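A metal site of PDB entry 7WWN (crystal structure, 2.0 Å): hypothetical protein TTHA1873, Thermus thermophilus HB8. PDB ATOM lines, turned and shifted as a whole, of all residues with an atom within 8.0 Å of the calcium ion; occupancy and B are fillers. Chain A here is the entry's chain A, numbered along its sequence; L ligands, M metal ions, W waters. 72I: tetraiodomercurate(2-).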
ATOM      1  N   LEU A  94      13.647  21.956  -6.049  1.00  0.00           N
ATOM      2  CA  LEU A  94      12.520  22.914  -6.186  1.00  0.00           C
ATOM      3  C   LEU A  94      13.091  24.277  -6.556  1.00  0.00           C
ATOM      4  O   LEU A  94      14.081  24.701  -5.944  1.00  0.00           O
ATOM      5  CB  LEU A  94      11.739  22.976  -4.870  1.00  0.00           C
ATOM      6  CG  LEU A  94      10.627  24.024  -4.756  1.00  0.00           C
ATOM      7  CD1 LEU A  94       9.458  23.735  -5.701  1.00  0.00           C
ATOM      8  CD2 LEU A  94      10.135  24.099  -3.305  1.00  0.00           C
ATOM      9  N   ASP A  95      12.528  24.888  -7.599  1.00  0.00           N
ATOM     10  CA  ASP A  95      12.675  26.333  -7.910  1.00  0.00           C
ATOM     11  C   ASP A  95      11.375  26.960  -7.470  1.00  0.00           C
ATOM     12  O   ASP A  95      10.392  26.895  -8.202  1.00  0.00           O
ATOM     13  CB  ASP A  95      13.002  26.611  -9.370  1.00  0.00           C
ATOM     14  CG  ASP A  95      13.207  28.106  -9.644  1.00  0.00           C
ATOM     15  OD1 ASP A  95      12.776  28.916  -8.800  1.00  0.00           O
ATOM     16  OD2 ASP A  95      13.782  28.436 -10.688  1.00  0.00           O
ATOM     17  N   PRO A  96      11.341  27.570  -6.264  1.00  0.00           N
ATOM     18  CA  PRO A  96      10.084  27.950  -5.623  1.00  0.00           C
ATOM     19  C   PRO A  96       9.248  28.987  -6.394  1.00  0.00           C
ATOM     20  O   PRO A  96       8.064  29.019  -6.165  1.00  0.00           O
ATOM     21  CB  PRO A  96      10.488  28.585  -4.267  1.00  0.00           C
ATOM     22  CG  PRO A  96      11.973  28.254  -4.088  1.00  0.00           C
ATOM     23  CD  PRO A  96      12.509  27.925  -5.462  1.00  0.00           C
ATOM     24  N   ASP A  97       9.874  29.809  -7.251  1.00  0.00           N
ATOM     25  CA  ASP A  97       9.178  30.878  -8.018  1.00  0.00           C
ATOM     26  C   ASP A  97       9.273  30.579  -9.509  1.00  0.00           C
ATOM     27  O   ASP A  97       8.798  31.402 -10.319  1.00  0.00           O
ATOM     28  CB  ASP A  97       9.729  32.267  -7.675  1.00  0.00           C
ATOM     29  CG  ASP A  97      11.236  32.392  -7.699  1.00  0.00           C
ATOM     30  OD1 ASP A  97      11.865  31.645  -8.449  1.00  0.00           O
ATOM     31  OD2 ASP A  97      11.772  33.281  -7.023  1.00  0.00           O
ATOM     32  N   GLY A  98       9.841  29.418  -9.851  1.00  0.00           N
ATOM     33  CA  GLY A  98       9.939  28.971 -11.250  1.00  0.00           C
ATOM     34  C   GLY A  98      10.798  29.962 -12.019  1.00  0.00           C
ATOM     35  O   GLY A  98      11.669  30.625 -11.442  1.00  0.00           O
ATOM     36  N   PRO A  99      10.544  30.100 -13.338  1.00  0.00           N
ATOM     37  CA  PRO A  99      11.228  31.120 -14.136  1.00  0.00           C
ATOM     38  C   PRO A  99      10.780  32.553 -13.824  1.00  0.00           C
ATOM     39  O   PRO A  99      11.361  33.464 -14.346  1.00  0.00           O
ATOM     40  CB  PRO A  99      10.837  30.746 -15.574  1.00  0.00           C
ATOM     41  CG  PRO A  99       9.475  30.101 -15.418  1.00  0.00           C
ATOM     42  CD  PRO A  99       9.599  29.305 -14.135  1.00  0.00           C
ATOM     43  N   PHE A 100       9.776  32.739 -12.987  1.00  0.00           N
ATOM     44  CA  PHE A 100       9.142  34.073 -12.793  1.00  0.00           C
ATOM     45  C   PHE A 100       9.871  34.891 -11.720  1.00  0.00           C
ATOM     46  O   PHE A 100       9.565  36.073 -11.590  1.00  0.00           O
ATOM     47  CB  PHE A 100       7.658  33.895 -12.457  1.00  0.00           C
ATOM     48  CG  PHE A 100       6.964  33.053 -13.485  1.00  0.00           C
ATOM     49  CD1 PHE A 100       6.639  33.569 -14.732  1.00  0.00           C
ATOM     50  CD2 PHE A 100       6.679  31.718 -13.236  1.00  0.00           C
ATOM     51  CE1 PHE A 100       6.036  32.775 -15.697  1.00  0.00           C
ATOM     52  CE2 PHE A 100       6.053  30.932 -14.199  1.00  0.00           C
ATOM     53  CZ  PHE A 100       5.727  31.463 -15.419  1.00  0.00           C
ATOM     54  N   GLY A 101      10.796  34.276 -10.984  1.00  0.00           N
ATOM     55  CA  GLY A 101      11.514  34.935  -9.884  1.00  0.00           C
ATOM     56  C   GLY A 101      12.943  34.426  -9.769  1.00  0.00           C
ATOM     57  O   GLY A 101      13.289  33.409 -10.349  1.00  0.00           O
ATOM     58  N   PRO A 102      13.810  35.129  -9.016  1.00  0.00           N
ATOM     59  CA  PRO A 102      15.244  34.856  -9.016  1.00  0.00           C
ATOM     60  C   PRO A 102      15.689  33.724  -8.085  1.00  0.00           C
ATOM     61  O   PRO A 102      16.853  33.396  -8.096  1.00  0.00           O
ATOM     62  CB  PRO A 102      15.850  36.179  -8.504  1.00  0.00           C
ATOM     63  CG  PRO A 102      14.790  36.658  -7.505  1.00  0.00           C
ATOM     64  CD  PRO A 102      13.461  36.254  -8.122  1.00  0.00           C
ATOM     65  N   ALA A 103      14.791  33.189  -7.267  1.00  0.00           N
ATOM     66  CA  ALA A 103      15.130  32.009  -6.463  1.00  0.00           C
ATOM     67  C   ALA A 103      15.679  30.932  -7.412  1.00  0.00           C
ATOM     68  O   ALA A 103      15.211  30.863  -8.595  1.00  0.00           O
ATOM     69  CB  ALA A 103      13.938  31.528  -5.701  1.00  0.00           C
ATOM     70  N   SER A 104      16.641  30.151  -6.920  1.00  0.00           N
ATOM     71  CA  SER A 104      17.290  29.061  -7.681  1.00  0.00           C
ATOM     72  C   SER A 104      16.779  27.705  -7.203  1.00  0.00           C
ATOM     73  O   SER A 104      16.182  27.610  -6.117  1.00  0.00           O
ATOM     74  CB  SER A 104      18.773  29.096  -7.556  1.00  0.00           C
ATOM     75  OG  SER A 104      19.251  30.396  -7.793  1.00  0.00           O
ATOM     76  N   TYR A 105      17.106  26.690  -7.982  1.00  0.00           N
ATOM     77  CA  TYR A 105      16.896  25.256  -7.653  1.00  0.00           C
ATOM     78  C   TYR A 105      17.705  24.898  -6.409  1.00  0.00           C
ATOM     79  O   TYR A 105      18.872  25.270  -6.276  1.00  0.00           O
ATOM     80  CB  TYR A 105      17.287  24.359  -8.837  1.00  0.00           C
ATOM     81  CG  TYR A 105      16.166  24.121  -9.816  1.00  0.00           C
ATOM     82  CD1 TYR A 105      15.029  23.437  -9.432  1.00  0.00           C
ATOM     83  CD2 TYR A 105      16.246  24.564 -11.129  1.00  0.00           C
ATOM     84  CE1 TYR A 105      14.000  23.202 -10.323  1.00  0.00           C
ATOM     85  CE2 TYR A 105      15.222  24.321 -12.031  1.00  0.00           C
ATOM     86  CZ  TYR A 105      14.084  23.653 -11.621  1.00  0.00           C
ATOM     87  OH  TYR A 105      13.071  23.397 -12.499  1.00  0.00           O
ATOM     88  N   GLY A 134       3.368  28.324 -10.728  1.00  0.00           N
ATOM     89  CA  GLY A 134       4.587  28.951 -11.267  1.00  0.00           C
ATOM     90  C   GLY A 134       5.848  28.205 -10.877  1.00  0.00           C
ATOM     91  O   GLY A 134       6.830  28.313 -11.604  1.00  0.00           O
ATOM     92  N   ALA A 135       5.822  27.477  -9.770  1.00  0.00           N
ATOM     93  CA  ALA A 135       7.007  26.754  -9.264  1.00  0.00           C
ATOM     94  C   ALA A 135       7.289  25.566 -10.180  1.00  0.00           C
ATOM     95  O   ALA A 135       6.356  25.100 -10.866  1.00  0.00           O
ATOM     96  CB  ALA A 135       6.814  26.303  -7.848  1.00  0.00           C
ATOM     97  N   THR A 136       8.532  25.088 -10.166  1.00  0.00           N
ATOM     98  CA  THR A 136       9.003  23.967 -11.015  1.00  0.00           C
ATOM     99  C   THR A 136       9.798  23.003 -10.157  1.00  0.00           C
ATOM    100  O   THR A 136      10.497  23.454  -9.223  1.00  0.00           O
ATOM    101  CB  THR A 136       9.850  24.460 -12.201  1.00  0.00           C
ATOM    102  OG1 THR A 136      11.121  24.871 -11.721  1.00  0.00           O
ATOM    103  CG2 THR A 136       9.203  25.593 -12.955  1.00  0.00           C
HETATM  104 HG1  72I L   1      10.773  34.438  -5.096  1.00  0.00          HG
HETATM  105  I1  72I L   1       9.524  32.310  -3.757  1.00  0.00           I
HETATM  106  I2  72I L   1       9.422  36.285  -6.687  1.00  0.00           I
HETATM  107  I3  72I L   1      13.007  35.344  -3.899  1.00  0.00           I
HETATM  108 CA    CA M   1      13.441  30.920  -9.918  1.00  0.00          CA
HETATM  109  O   HOH W   1      14.878  31.272 -11.785  1.00  0.00           O
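OD2 of Asp 97 binds HG1 of the ligand (2.5 Å).
The backbone carbonyl oxygen (O) of Thr 136 lies within hydrogen-bond range of the backbone NH (N) of Asp 95 (3.0 Å).
Of the 15 residues printed, 5 come within 4 Å of the calcium ion.
Along chain A the residues within 4 Å of the calcium ion span positions 95 to 103.
The calcium ion is bound by the backbone carbonyl oxygen (O) of Ala 103, the side-chain carboxylate (OD1) of Asp 97, the backbone carbonyl oxygen (O) of Gly 98, water W1, the side-chain carboxylate (OD1) of Asp 95, the backbone carbonyl oxygen (O) of Gly 101 and the side-chain carboxylate (OD2) of Asp 95.
The calcium ion has seven donor atoms within binding distance.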
